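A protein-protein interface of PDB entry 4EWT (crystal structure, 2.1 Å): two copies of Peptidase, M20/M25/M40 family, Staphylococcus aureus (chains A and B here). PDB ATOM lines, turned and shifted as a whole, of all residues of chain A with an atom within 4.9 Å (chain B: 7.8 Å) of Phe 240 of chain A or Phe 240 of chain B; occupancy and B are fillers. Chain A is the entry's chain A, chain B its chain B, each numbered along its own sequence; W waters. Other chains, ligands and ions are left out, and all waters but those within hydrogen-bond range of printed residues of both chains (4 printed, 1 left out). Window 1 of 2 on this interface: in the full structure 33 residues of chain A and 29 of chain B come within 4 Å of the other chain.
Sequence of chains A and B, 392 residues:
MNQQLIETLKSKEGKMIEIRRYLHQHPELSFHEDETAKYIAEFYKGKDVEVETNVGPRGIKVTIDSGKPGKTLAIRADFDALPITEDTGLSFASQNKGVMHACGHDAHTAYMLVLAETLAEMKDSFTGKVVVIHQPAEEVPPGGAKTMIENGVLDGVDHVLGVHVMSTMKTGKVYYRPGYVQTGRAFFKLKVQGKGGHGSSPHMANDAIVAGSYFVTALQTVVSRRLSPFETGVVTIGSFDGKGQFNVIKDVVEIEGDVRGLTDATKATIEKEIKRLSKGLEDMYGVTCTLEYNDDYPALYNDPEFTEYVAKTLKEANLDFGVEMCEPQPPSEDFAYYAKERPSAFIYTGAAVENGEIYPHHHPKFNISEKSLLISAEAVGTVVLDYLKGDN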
ATOM      1  N   ILE A 209     -24.299   5.105   7.933  1.00  0.00           N
ATOM      2  CA  ILE A 209     -24.069   6.560   7.880  1.00  0.00           C
ATOM      3  C   ILE A 209     -22.568   6.861   7.905  1.00  0.00           C
ATOM      4  O   ILE A 209     -22.097   7.673   7.138  1.00  0.00           O
ATOM      5  CB  ILE A 209     -24.864   7.328   8.971  1.00  0.00           C
ATOM      6  CG1 ILE A 209     -26.341   7.377   8.553  1.00  0.00           C
ATOM      7  CG2 ILE A 209     -24.290   8.761   9.190  1.00  0.00           C
ATOM      8  CD1 ILE A 209     -27.315   7.801   9.653  1.00  0.00           C
ATOM      9  N   GLY A 212     -21.163   5.764   4.490  1.00  0.00           N
ATOM     10  CA  GLY A 212     -21.580   6.703   3.453  1.00  0.00           C
ATOM     11  C   GLY A 212     -20.854   8.037   3.595  1.00  0.00           C
ATOM     12  O   GLY A 212     -20.495   8.659   2.589  1.00  0.00           O
ATOM     13  N   SER A 213     -20.624   8.458   4.842  1.00  0.00           N
ATOM     14  CA  SER A 213     -19.890   9.705   5.122  1.00  0.00           C
ATOM     15  C   SER A 213     -18.422   9.593   4.729  1.00  0.00           C
ATOM     16  O   SER A 213     -17.855  10.551   4.201  1.00  0.00           O
ATOM     17  CB  SER A 213     -19.991  10.078   6.590  1.00  0.00           C
ATOM     18  OG  SER A 213     -21.317  10.532   6.861  1.00  0.00           O
ATOM     19  N   VAL A 216     -18.327   9.937   1.007  1.00  0.00           N
ATOM     20  CA  VAL A 216     -18.439  11.313   0.506  1.00  0.00           C
ATOM     21  C   VAL A 216     -17.083  12.021   0.583  1.00  0.00           C
ATOM     22  O   VAL A 216     -16.698  12.669  -0.381  1.00  0.00           O
ATOM     23  CB  VAL A 216     -19.586  12.133   1.195  1.00  0.00           C
ATOM     24  CG1 VAL A 216     -19.563  13.591   0.780  1.00  0.00           C
ATOM     25  CG2 VAL A 216     -20.983  11.519   0.862  1.00  0.00           C
ATOM     26  N   ILE A 237     -22.769  15.157  -4.777  1.00  0.00           N
ATOM     27  CA  ILE A 237     -23.750  14.326  -4.087  1.00  0.00           C
ATOM     28  C   ILE A 237     -24.848  15.265  -3.641  1.00  0.00           C
ATOM     29  O   ILE A 237     -24.681  15.988  -2.667  1.00  0.00           O
ATOM     30  CB  ILE A 237     -23.204  13.582  -2.844  1.00  0.00           C
ATOM     31  CG1 ILE A 237     -22.067  12.629  -3.211  1.00  0.00           C
ATOM     32  CG2 ILE A 237     -24.333  12.793  -2.157  1.00  0.00           C
ATOM     33  CD1 ILE A 237     -22.457  11.559  -4.256  1.00  0.00           C
ATOM     34  N   GLY A 238     -25.967  15.255  -4.368  1.00  0.00           N
ATOM     35  CA  GLY A 238     -27.091  16.103  -4.049  1.00  0.00           C
ATOM     36  C   GLY A 238     -28.078  15.500  -3.067  1.00  0.00           C
ATOM     37  O   GLY A 238     -28.899  16.218  -2.491  1.00  0.00           O
ATOM     38  N   SER A 239     -27.999  14.188  -2.856  1.00  0.00           N
ATOM     39  CA  SER A 239     -28.940  13.522  -1.951  1.00  0.00           C
ATOM     40  C   SER A 239     -28.210  12.466  -1.123  1.00  0.00           C
ATOM     41  O   SER A 239     -27.637  11.522  -1.669  1.00  0.00           O
ATOM     42  CB  SER A 239     -30.089  12.908  -2.745  1.00  0.00           C
ATOM     43  OG  SER A 239     -31.124  12.493  -1.895  1.00  0.00           O
ATOM     44  N   PHE A 240     -28.169  12.678   0.194  1.00  0.00           N
ATOM     45  CA  PHE A 240     -27.636  11.680   1.113  1.00  0.00           C
ATOM     46  C   PHE A 240     -28.841  11.336   1.991  1.00  0.00           C
ATOM     47  O   PHE A 240     -29.137  12.039   2.964  1.00  0.00           O
ATOM     48  CB  PHE A 240     -26.471  12.291   1.912  1.00  0.00           C
ATOM     49  CG  PHE A 240     -25.702  11.301   2.799  1.00  0.00           C
ATOM     50  CD1 PHE A 240     -24.339  11.147   2.652  1.00  0.00           C
ATOM     51  CD2 PHE A 240     -26.331  10.593   3.813  1.00  0.00           C
ATOM     52  CE1 PHE A 240     -23.611  10.266   3.473  1.00  0.00           C
ATOM     53  CE2 PHE A 240     -25.618   9.696   4.635  1.00  0.00           C
ATOM     54  CZ  PHE A 240     -24.262   9.540   4.466  1.00  0.00           C
ATOM     55  N   ASP A 241     -29.585  10.301   1.605  1.00  0.00           N
ATOM     56  CA  ASP A 241     -30.795   9.963   2.340  1.00  0.00           C
ATOM     57  C   ASP A 241     -30.471   8.982   3.448  1.00  0.00           C
ATOM     58  O   ASP A 241     -30.420   7.788   3.225  1.00  0.00           O
ATOM     59  CB  ASP A 241     -31.900   9.461   1.405  1.00  0.00           C
ATOM     60  CG  ASP A 241     -33.228   9.253   2.116  1.00  0.00           C
ATOM     61  OD1 ASP A 241     -33.440   9.793   3.233  1.00  0.00           O
ATOM     62  OD2 ASP A 241     -34.079   8.537   1.549  1.00  0.00           O
ATOM     63  N   GLY A 242     -30.215   9.526   4.642  1.00  0.00           N
ATOM     64  CA  GLY A 242     -29.859   8.738   5.827  1.00  0.00           C
ATOM     65  C   GLY A 242     -30.731   9.036   7.043  1.00  0.00           C
ATOM     66  O   GLY A 242     -30.302   8.842   8.186  1.00  0.00           O
ATOM     67  N   LYS A 243     -31.944   9.522   6.806  1.00  0.00           N
ATOM     68  CA  LYS A 243     -32.855   9.846   7.895  1.00  0.00           C
ATOM     69  C   LYS A 243     -33.238   8.579   8.668  1.00  0.00           C
ATOM     70  O   LYS A 243     -33.533   7.539   8.090  1.00  0.00           O
ATOM     71  CB  LYS A 243     -34.095  10.586   7.399  1.00  0.00           C
ATOM     72  CG  LYS A 243     -34.980  11.095   8.559  1.00  0.00           C
ATOM     73  CD  LYS A 243     -36.232  11.761   8.049  1.00  0.00           C
ATOM     74  CE  LYS A 243     -37.203  12.086   9.206  1.00  0.00           C
ATOM     75  NZ  LYS A 243     -36.474  12.744  10.363  1.00  0.00           N
ATOM     76  N   GLY A 244     -33.202   8.668   9.985  1.00  0.00           N
ATOM     77  CA  GLY A 244     -33.420   7.492  10.799  1.00  0.00           C
ATOM     78  C   GLY A 244     -33.965   7.871  12.145  1.00  0.00           C
ATOM     79  O   GLY A 244     -34.607   8.901  12.292  1.00  0.00           O
ATOM     80  N   VAL A 253     -28.095   3.643   3.750  1.00  0.00           N
ATOM     81  CA  VAL A 253     -28.229   5.006   3.242  1.00  0.00           C
ATOM     82  C   VAL A 253     -28.346   4.988   1.709  1.00  0.00           C
ATOM     83  O   VAL A 253     -27.776   4.130   1.027  1.00  0.00           O
ATOM     84  CB  VAL A 253     -27.128   6.018   3.751  1.00  0.00           C
ATOM     85  CG1 VAL A 253     -26.988   6.003   5.290  1.00  0.00           C
ATOM     86  CG2 VAL A 253     -25.802   5.780   3.116  1.00  0.00           C
ATOM     87  N   GLU A 254     -29.125   5.880   1.148  1.00  0.00           N
ATOM     88  CA  GLU A 254     -29.192   6.051  -0.281  1.00  0.00           C
ATOM     89  C   GLU A 254     -28.587   7.342  -0.700  1.00  0.00           C
ATOM     90  O   GLU A 254     -28.972   8.371  -0.277  1.00  0.00           O
ATOM     91  CB  GLU A 254     -30.597   6.028  -0.832  1.00  0.00           C
ATOM     92  CG  GLU A 254     -31.387   4.908  -0.435  1.00  0.00           C
ATOM     93  CD  GLU A 254     -31.317   3.763  -1.346  1.00  0.00           C
ATOM     94  OE1 GLU A 254     -30.628   3.813  -2.362  1.00  0.00           O
ATOM     95  OE2 GLU A 254     -31.950   2.779  -1.007  1.00  0.00           O
ATOM     96  N   ILE A 255     -27.624   7.230  -1.563  1.00  0.00           N
ATOM     97  CA  ILE A 255     -26.913   8.377  -2.076  1.00  0.00           C
ATOM     98  C   ILE A 255     -27.270   8.580  -3.543  1.00  0.00           C
ATOM     99  O   ILE A 255     -27.305   7.629  -4.315  1.00  0.00           O
ATOM    100  CB  ILE A 255     -25.390   8.220  -1.887  1.00  0.00           C
ATOM    101  CG1 ILE A 255     -25.008   8.523  -0.425  1.00  0.00           C
ATOM    102  CG2 ILE A 255     -24.618   9.100  -2.885  1.00  0.00           C
ATOM    103  CD1 ILE A 255     -23.738   7.782   0.033  1.00  0.00           C
ATOM    104  N   VAL B 192     -26.696  21.656  10.029  1.00  0.00           N
ATOM    105  CA  VAL B 192     -25.571  22.154   9.248  1.00  0.00           C
ATOM    106  C   VAL B 192     -26.089  22.972   8.036  1.00  0.00           C
ATOM    107  O   VAL B 192     -26.604  22.404   7.060  1.00  0.00           O
ATOM    108  CB  VAL B 192     -24.693  20.978   8.756  1.00  0.00           C
ATOM    109  CG1 VAL B 192     -23.455  21.475   7.969  1.00  0.00           C
ATOM    110  CG2 VAL B 192     -24.264  20.068   9.950  1.00  0.00           C
ATOM    111  N   ALA B 208     -23.563  21.419   2.076  1.00  0.00           N
ATOM    112  CA  ALA B 208     -23.825  20.936   3.436  1.00  0.00           C
ATOM    113  C   ALA B 208     -23.676  19.408   3.586  1.00  0.00           C
ATOM    114  O   ALA B 208     -23.415  18.932   4.670  1.00  0.00           O
ATOM    115  CB  ALA B 208     -25.191  21.406   3.956  1.00  0.00           C
ATOM    116  N   ILE B 209     -23.843  18.655   2.504  1.00  0.00           N
ATOM    117  CA  ILE B 209     -23.623  17.193   2.544  1.00  0.00           C
ATOM    118  C   ILE B 209     -22.122  16.865   2.770  1.00  0.00           C
ATOM    119  O   ILE B 209     -21.761  15.985   3.570  1.00  0.00           O
ATOM    120  CB  ILE B 209     -24.187  16.481   1.279  1.00  0.00           C
ATOM    121  CG1 ILE B 209     -25.704  16.370   1.400  1.00  0.00           C
ATOM    122  CG2 ILE B 209     -23.625  15.047   1.135  1.00  0.00           C
ATOM    123  CD1 ILE B 209     -26.430  15.939   0.092  1.00  0.00           C
ATOM    124  N   VAL B 210     -21.260  17.595   2.067  1.00  0.00           N
ATOM    125  CA  VAL B 210     -19.823  17.472   2.249  1.00  0.00           C
ATOM    126  C   VAL B 210     -19.416  17.894   3.694  1.00  0.00           C
ATOM    127  O   VAL B 210     -18.689  17.162   4.382  1.00  0.00           O
ATOM    128  CB  VAL B 210     -19.085  18.283   1.181  1.00  0.00           C
ATOM    129  CG1 VAL B 210     -17.591  18.486   1.554  1.00  0.00           C
ATOM    130  CG2 VAL B 210     -19.251  17.648  -0.183  1.00  0.00           C
ATOM    131  N   ALA B 211     -19.901  19.048   4.155  1.00  0.00           N
ATOM    132  CA  ALA B 211     -19.560  19.501   5.520  1.00  0.00           C
ATOM    133  C   ALA B 211     -20.020  18.454   6.540  1.00  0.00           C
ATOM    134  O   ALA B 211     -19.259  18.044   7.411  1.00  0.00           O
ATOM    135  CB  ALA B 211     -20.183  20.847   5.825  1.00  0.00           C
ATOM    136  N   GLY B 212     -21.266  18.017   6.397  1.00  0.00           N
ATOM    137  CA  GLY B 212     -21.832  17.027   7.297  1.00  0.00           C
ATOM    138  C   GLY B 212     -21.079  15.710   7.270  1.00  0.00           C
ATOM    139  O   GLY B 212     -20.859  15.092   8.309  1.00  0.00           O
ATOM    140  N   SER B 213     -20.702  15.270   6.078  1.00  0.00           N
ATOM    141  CA  SER B 213     -19.930  14.038   5.923  1.00  0.00           C
ATOM    142  C   SER B 213     -18.569  14.129   6.628  1.00  0.00           C
ATOM    143  O   SER B 213     -18.144  13.186   7.310  1.00  0.00           O
ATOM    144  CB  SER B 213     -19.735  13.720   4.450  1.00  0.00           C
ATOM    145  OG  SER B 213     -20.943  13.153   3.908  1.00  0.00           O
ATOM    146  N   TYR B 214     -17.855  15.210   6.413  1.00  0.00           N
ATOM    147  CA  TYR B 214     -16.640  15.504   7.092  1.00  0.00           C
ATOM    148  C   TYR B 214     -16.877  15.553   8.656  1.00  0.00           C
ATOM    149  O   TYR B 214     -16.105  14.998   9.351  1.00  0.00           O
ATOM    150  CB  TYR B 214     -15.852  16.684   6.506  1.00  0.00           C
ATOM    151  CG  TYR B 214     -15.007  16.385   5.223  1.00  0.00           C
ATOM    152  CD1 TYR B 214     -13.693  15.912   5.292  1.00  0.00           C
ATOM    153  CD2 TYR B 214     -15.534  16.554   3.948  1.00  0.00           C
ATOM    154  CE1 TYR B 214     -12.967  15.659   4.124  1.00  0.00           C
ATOM    155  CE2 TYR B 214     -14.803  16.331   2.803  1.00  0.00           C
ATOM    156  CZ  TYR B 214     -13.539  15.870   2.867  1.00  0.00           C
ATOM    157  OH  TYR B 214     -12.884  15.598   1.716  1.00  0.00           O
ATOM    158  N   PHE B 215     -17.968  16.130   9.093  1.00  0.00           N
ATOM    159  CA  PHE B 215     -18.305  16.160  10.518  1.00  0.00           C
ATOM    160  C   PHE B 215     -18.369  14.719  11.079  1.00  0.00           C
ATOM    161  O   PHE B 215     -17.756  14.428  12.098  1.00  0.00           O
ATOM    162  CB  PHE B 215     -19.625  16.902  10.799  1.00  0.00           C
ATOM    163  CG  PHE B 215     -20.043  16.859  12.243  1.00  0.00           C
ATOM    164  CD1 PHE B 215     -19.434  17.680  13.185  1.00  0.00           C
ATOM    165  CD2 PHE B 215     -21.033  15.971  12.671  1.00  0.00           C
ATOM    166  CE1 PHE B 215     -19.802  17.609  14.513  1.00  0.00           C
ATOM    167  CE2 PHE B 215     -21.414  15.917  13.991  1.00  0.00           C
ATOM    168  CZ  PHE B 215     -20.790  16.733  14.917  1.00  0.00           C
ATOM    169  N   VAL B 216     -19.076  13.826  10.389  1.00  0.00           N
ATOM    170  CA  VAL B 216     -19.287  12.469  10.907  1.00  0.00           C
ATOM    171  C   VAL B 216     -17.956  11.712  11.021  1.00  0.00           C
ATOM    172  O   VAL B 216     -17.745  10.873  11.905  1.00  0.00           O
ATOM    173  CB  VAL B 216     -20.275  11.691  10.004  1.00  0.00           C
ATOM    174  CG1 VAL B 216     -20.273  10.184  10.330  1.00  0.00           C
ATOM    175  CG2 VAL B 216     -21.681  12.296  10.148  1.00  0.00           C
ATOM    176  N   THR B 217     -17.074  12.038  10.097  1.00  0.00           N
ATOM    177  CA  THR B 217     -15.757  11.483  10.000  1.00  0.00           C
ATOM    178  C   THR B 217     -14.904  11.927  11.181  1.00  0.00           C
ATOM    179  O   THR B 217     -14.330  11.091  11.874  1.00  0.00           O
ATOM    180  CB  THR B 217     -15.222  11.932   8.609  1.00  0.00           C
ATOM    181  OG1 THR B 217     -15.344  10.858   7.690  1.00  0.00           O
ATOM    182  CG2 THR B 217     -13.877  12.467   8.615  1.00  0.00           C
ATOM    183  N   ILE B 237     -24.371   8.579  15.196  1.00  0.00           N
ATOM    184  CA  ILE B 237     -25.272   9.406  14.398  1.00  0.00           C
ATOM    185  C   ILE B 237     -26.297   8.466  13.766  1.00  0.00           C
ATOM    186  O   ILE B 237     -25.958   7.708  12.854  1.00  0.00           O
ATOM    187  CB  ILE B 237     -24.531  10.200  13.285  1.00  0.00           C
ATOM    188  CG1 ILE B 237     -23.488  11.153  13.884  1.00  0.00           C
ATOM    189  CG2 ILE B 237     -25.523  10.969  12.445  1.00  0.00           C
ATOM    190  CD1 ILE B 237     -24.043  12.145  14.916  1.00  0.00           C
ATOM    191  N   GLY B 238     -27.541   8.514  14.243  1.00  0.00           N
ATOM    192  CA  GLY B 238     -28.586   7.604  13.739  1.00  0.00           C
ATOM    193  C   GLY B 238     -29.375   8.175  12.571  1.00  0.00           C
ATOM    194  O   GLY B 238     -30.062   7.451  11.864  1.00  0.00           O
ATOM    195  N   SER B 239     -29.276   9.489  12.374  1.00  0.00           N
ATOM    196  CA  SER B 239     -30.028  10.179  11.358  1.00  0.00           C
ATOM    197  C   SER B 239     -29.162  11.211  10.653  1.00  0.00           C
ATOM    198  O   SER B 239     -28.580  12.107  11.293  1.00  0.00           O
ATOM    199  CB  SER B 239     -31.267  10.831  11.987  1.00  0.00           C
ATOM    200  OG  SER B 239     -32.199  11.269  10.993  1.00  0.00           O
ATOM    201  N   PHE B 240     -29.034  11.062   9.337  1.00  0.00           N
ATOM    202  CA  PHE B 240     -28.310  12.036   8.527  1.00  0.00           C
ATOM    203  C   PHE B 240     -29.280  12.370   7.403  1.00  0.00           C
ATOM    204  O   PHE B 240     -29.395  11.647   6.392  1.00  0.00           O
ATOM    205  CB  PHE B 240     -26.982  11.437   8.019  1.00  0.00           C
ATOM    206  CG  PHE B 240     -26.116  12.402   7.235  1.00  0.00           C
ATOM    207  CD1 PHE B 240     -24.790  12.629   7.609  1.00  0.00           C
ATOM    208  CD2 PHE B 240     -26.599  13.045   6.085  1.00  0.00           C
ATOM    209  CE1 PHE B 240     -23.969  13.510   6.861  1.00  0.00           C
ATOM    210  CE2 PHE B 240     -25.785  13.920   5.334  1.00  0.00           C
ATOM    211  CZ  PHE B 240     -24.474  14.164   5.735  1.00  0.00           C
ATOM    212  N   ASP B 241     -30.026  13.441   7.614  1.00  0.00           N
ATOM    213  CA  ASP B 241     -31.132  13.792   6.732  1.00  0.00           C
ATOM    214  C   ASP B 241     -30.631  14.793   5.711  1.00  0.00           C
ATOM    215  O   ASP B 241     -30.655  15.997   5.954  1.00  0.00           O
ATOM    216  CB  ASP B 241     -32.293  14.366   7.546  1.00  0.00           C
ATOM    217  CG  ASP B 241     -33.526  14.680   6.698  1.00  0.00           C
ATOM    218  OD1 ASP B 241     -33.626  14.239   5.530  1.00  0.00           O
ATOM    219  OD2 ASP B 241     -34.428  15.364   7.219  1.00  0.00           O
ATOM    220  N   GLY B 242     -30.183  14.272   4.568  1.00  0.00           N
ATOM    221  CA  GLY B 242     -29.591  15.084   3.511  1.00  0.00           C
ATOM    222  C   GLY B 242     -30.279  14.771   2.187  1.00  0.00           C
ATOM    223  O   GLY B 242     -29.727  14.978   1.113  1.00  0.00           O
ATOM    224  N   LYS B 243     -31.497  14.258   2.283  1.00  0.00           N
ATOM    225  CA  LYS B 243     -32.298  13.920   1.115  1.00  0.00           C
ATOM    226  C   LYS B 243     -32.538  15.163   0.240  1.00  0.00           C
ATOM    227  O   LYS B 243     -32.922  16.229   0.735  1.00  0.00           O
ATOM    228  CB  LYS B 243     -33.605  13.292   1.574  1.00  0.00           C
ATOM    229  CG  LYS B 243     -34.682  13.217   0.529  1.00  0.00           C
ATOM    230  CD  LYS B 243     -34.493  12.029  -0.355  1.00  0.00           C
ATOM    231  CE  LYS B 243     -35.829  11.616  -0.953  1.00  0.00           C
ATOM    232  NZ  LYS B 243     -35.579  10.911  -2.245  1.00  0.00           N
ATOM    233  N   GLY B 244     -32.296  15.017  -1.056  1.00  0.00           N
ATOM    234  CA  GLY B 244     -32.362  16.147  -1.960  1.00  0.00           C
ATOM    235  C   GLY B 244     -32.685  15.826  -3.401  1.00  0.00           C
ATOM    236  O   GLY B 244     -33.397  14.864  -3.697  1.00  0.00           O
ATOM    237  N   GLN B 245     -32.173  16.657  -4.287  1.00  0.00           N
ATOM    238  CA  GLN B 245     -32.390  16.548  -5.702  1.00  0.00           C
ATOM    239  C   GLN B 245     -31.081  16.267  -6.373  1.00  0.00           C
ATOM    240  O   GLN B 245     -30.097  16.812  -5.989  1.00  0.00           O
ATOM    241  CB  GLN B 245     -32.947  17.841  -6.270  1.00  0.00           C
ATOM    242  CG  GLN B 245     -34.134  18.392  -5.547  1.00  0.00           C
ATOM    243  CD  GLN B 245     -34.445  19.843  -5.943  1.00  0.00           C
ATOM    244  OE1 GLN B 245     -34.992  20.080  -7.018  1.00  0.00           O
ATOM    245  NE2 GLN B 245     -34.083  20.821  -5.081  1.00  0.00           N
ATOM    246  N   LYS B 250     -26.782  20.632  -1.951  1.00  0.00           N
ATOM    247  CA  LYS B 250     -27.713  20.647  -0.835  1.00  0.00           C
ATOM    248  C   LYS B 250     -27.406  21.763   0.148  1.00  0.00           C
ATOM    249  O   LYS B 250     -26.258  21.906   0.588  1.00  0.00           O
ATOM    250  CB  LYS B 250     -27.694  19.291  -0.140  1.00  0.00           C
ATOM    251  CG  LYS B 250     -28.727  19.127   0.967  1.00  0.00           C
ATOM    252  CD  LYS B 250     -30.142  19.036   0.405  1.00  0.00           C
ATOM    253  CE  LYS B 250     -31.174  18.861   1.502  1.00  0.00           C
ATOM    254  NZ  LYS B 250     -32.544  18.865   0.926  1.00  0.00           N
ATOM    255  N   VAL B 252     -28.742  22.425   3.315  1.00  0.00           N
ATOM    256  CA  VAL B 252     -28.822  22.168   4.744  1.00  0.00           C
ATOM    257  C   VAL B 252     -28.900  20.664   4.949  1.00  0.00           C
ATOM    258  O   VAL B 252     -29.512  19.961   4.139  1.00  0.00           O
ATOM    259  CB  VAL B 252     -30.022  22.933   5.417  1.00  0.00           C
ATOM    260  CG1 VAL B 252     -31.328  22.673   4.702  1.00  0.00           C
ATOM    261  CG2 VAL B 252     -30.162  22.597   6.905  1.00  0.00           C
ATOM    262  N   VAL B 253     -28.230  20.159   5.976  1.00  0.00           N
ATOM    263  CA  VAL B 253     -28.548  18.806   6.442  1.00  0.00           C
ATOM    264  C   VAL B 253     -28.894  18.813   7.930  1.00  0.00           C
ATOM    265  O   VAL B 253     -28.389  19.644   8.696  1.00  0.00           O
ATOM    266  CB  VAL B 253     -27.462  17.703   6.123  1.00  0.00           C
ATOM    267  CG1 VAL B 253     -27.081  17.678   4.629  1.00  0.00           C
ATOM    268  CG2 VAL B 253     -26.221  17.839   7.011  1.00  0.00           C
ATOM    269  N   GLU B 254     -29.746  17.875   8.318  1.00  0.00           N
ATOM    270  CA  GLU B 254     -30.092  17.680   9.721  1.00  0.00           C
ATOM    271  C   GLU B 254     -29.477  16.382  10.229  1.00  0.00           C
ATOM    272  O   GLU B 254     -29.764  15.287   9.719  1.00  0.00           O
ATOM    273  CB  GLU B 254     -31.616  17.660   9.927  1.00  0.00           C
ATOM    274  CG  GLU B 254     -32.355  18.890   9.393  1.00  0.00           C
ATOM    275  CD  GLU B 254     -32.254  20.120  10.303  1.00  0.00           C
ATOM    276  OE1 GLU B 254     -31.593  20.059  11.370  1.00  0.00           O
ATOM    277  OE2 GLU B 254     -32.861  21.158   9.949  1.00  0.00           O
ATOM    278  N   ILE B 255     -28.624  16.522  11.228  1.00  0.00           N
ATOM    279  CA  ILE B 255     -27.974  15.396  11.868  1.00  0.00           C
ATOM    280  C   ILE B 255     -28.548  15.172  13.269  1.00  0.00           C
ATOM    281  O   ILE B 255     -28.746  16.126  14.017  1.00  0.00           O
ATOM    282  CB  ILE B 255     -26.447  15.586  11.883  1.00  0.00           C
ATOM    283  CG1 ILE B 255     -25.878  15.097  10.534  1.00  0.00           C
ATOM    284  CG2 ILE B 255     -25.810  14.795  13.021  1.00  0.00           C
ATOM    285  CD1 ILE B 255     -24.588  15.793  10.095  1.00  0.00           C
ATOM    286  N   GLU B 256     -28.894  13.926  13.588  1.00  0.00           N
ATOM    287  CA  GLU B 256     -29.330  13.608  14.951  1.00  0.00           C
ATOM    288  C   GLU B 256     -28.430  12.527  15.542  1.00  0.00           C
ATOM    289  O   GLU B 256     -28.083  11.558  14.876  1.00  0.00           O
ATOM    290  CB  GLU B 256     -30.811  13.205  15.003  1.00  0.00           C
ATOM    291  CG  GLU B 256     -31.751  14.285  14.468  1.00  0.00           C
ATOM    292  CD  GLU B 256     -33.225  13.959  14.618  1.00  0.00           C
ATOM    293  OE1 GLU B 256     -33.603  12.766  14.654  1.00  0.00           O
ATOM    294  OE2 GLU B 256     -34.022  14.911  14.693  1.00  0.00           O
ATOM    295  N   GLY B 257     -28.075  12.702  16.806  1.00  0.00           N
ATOM    296  CA  GLY B 257     -27.141  11.826  17.452  1.00  0.00           C
ATOM    297  C   GLY B 257     -27.609  11.338  18.800  1.00  0.00           C
ATOM    298  O   GLY B 257     -28.529  11.887  19.387  1.00  0.00           O
HETATM  299  O   HOH W   1     -29.820  18.651  -3.278  1.00  0.00           O
HETATM  300  O   HOH W   2     -34.105  15.122  10.402  1.00  0.00           O
HETATM  301  O   HOH W   3     -24.676  18.594  -2.019  1.00  0.00           O
HETATM  302  O   HOH W   4     -33.787  12.223  -3.644  1.00  0.00           O
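Water W4 lies within hydrogen-bond range of the side-chain amino group of Lys 243 of chain B, the backbone carbonyl oxygen of Gly 244 of chain B and the side-chain hydroxyl of Ser 239 of chain A.
Gly 238 of chain B touches Ile 209 of chain A. Ser 213 of chain A touches Phe 240 of chain B. O of Gly 238 of chain A touches O of Gly 242 of chain B, at 3.9 Å. CE1 of Phe 240 of chain A touches OG of Ser 213 of chain B, 3.96 Å away. Gly 242 of chain A touches Gly 238 of chain B (O to O, 3.9 Å).
Printed residues of chain B within 4 Å of Ser 213 of chain A: Ser 213 (3.7 Å), Val 216 (3.5 Å) and Phe 240 (3.99 Å). Of the printed residues of chain B, Asp 241 of chain A touches Lys 243. Of chain B, only Gly 238 (3.9 Å), Ser 239 (3.5 Å) and Phe 240 (2.8 Å) come within 4 Å of Gly 242 of chain A. Of the printed residues of chain A, Ser 213 of chain B touches Ser 213, Val 216 and Phe 240. The nearest residue of chain B that does not touch Phe 240 of chain A is Asp 241 of chain B (4.2 Å).
Of the 27 printed residues of chain B, 11 touch a printed residue of chain A. Hydrophobic or aromatic side chains of chain B that line the printed part of chain A: Ile 209, Val 216 and Phe 240. Hydrophobic or aromatic side chains of chain A that line the printed part of chain B: Ile 209, Val 216 and Phe 240. Among the printed residues, no Asp or Glu carboxylate lies within 4 Å of a Lys or Arg side-chain nitrogen of the other chain.
Ser 239 of chain A touches Gly 242 of chain B, and with the chains exchanged Gly 242 of chain A touches Ser 239 of chain B. Asp 241 of chain A touches Lys 243 of chain B, but with the chains exchanged Lys 243 of chain A does not touch Asp 241 of chain B (4.1 Å).
NZ of Lys 250 of chain B sits at hydrogen-bond distance from O of Lys 243 of chain B, at 2.7 Å. The backbone NH of Asp 241 of chain A lies within hydrogen-bond range of the backbone carbonyl oxygen of Glu 254 of chain A.
N of Phe 240 of chain A lies within hydrogen-bond range of O of Gly 242 of chain B, 2.9 Å away. N of Lys 243 of chain A is in hydrogen-bond range of O of Phe 240 of chain B. The backbone NH of Gly 244 of chain B is in hydrogen-bond range of the side-chain hydroxyl of Ser 239 of chain A (2.9 Å). The backbone carbonyl oxygen of Phe 240 of chain B lies close to the backbone carbonyl oxygen of Phe 240 of chain A, 3.5 Å away. N of Gly 244 of chain A sits at hydrogen-bond distance from OG of Ser 239 of chain B (3.0 Å). The backbone carbonyl oxygen of Phe 240 of chain A lies within hydrogen-bond range of the backbone NH of Lys 243 of chain B. The backbone NH (N) of Phe 240 of chain B sits at hydrogen-bond distance from the backbone carbonyl oxygen (O) of Gly 242 of chain A, at 2.8 Å.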
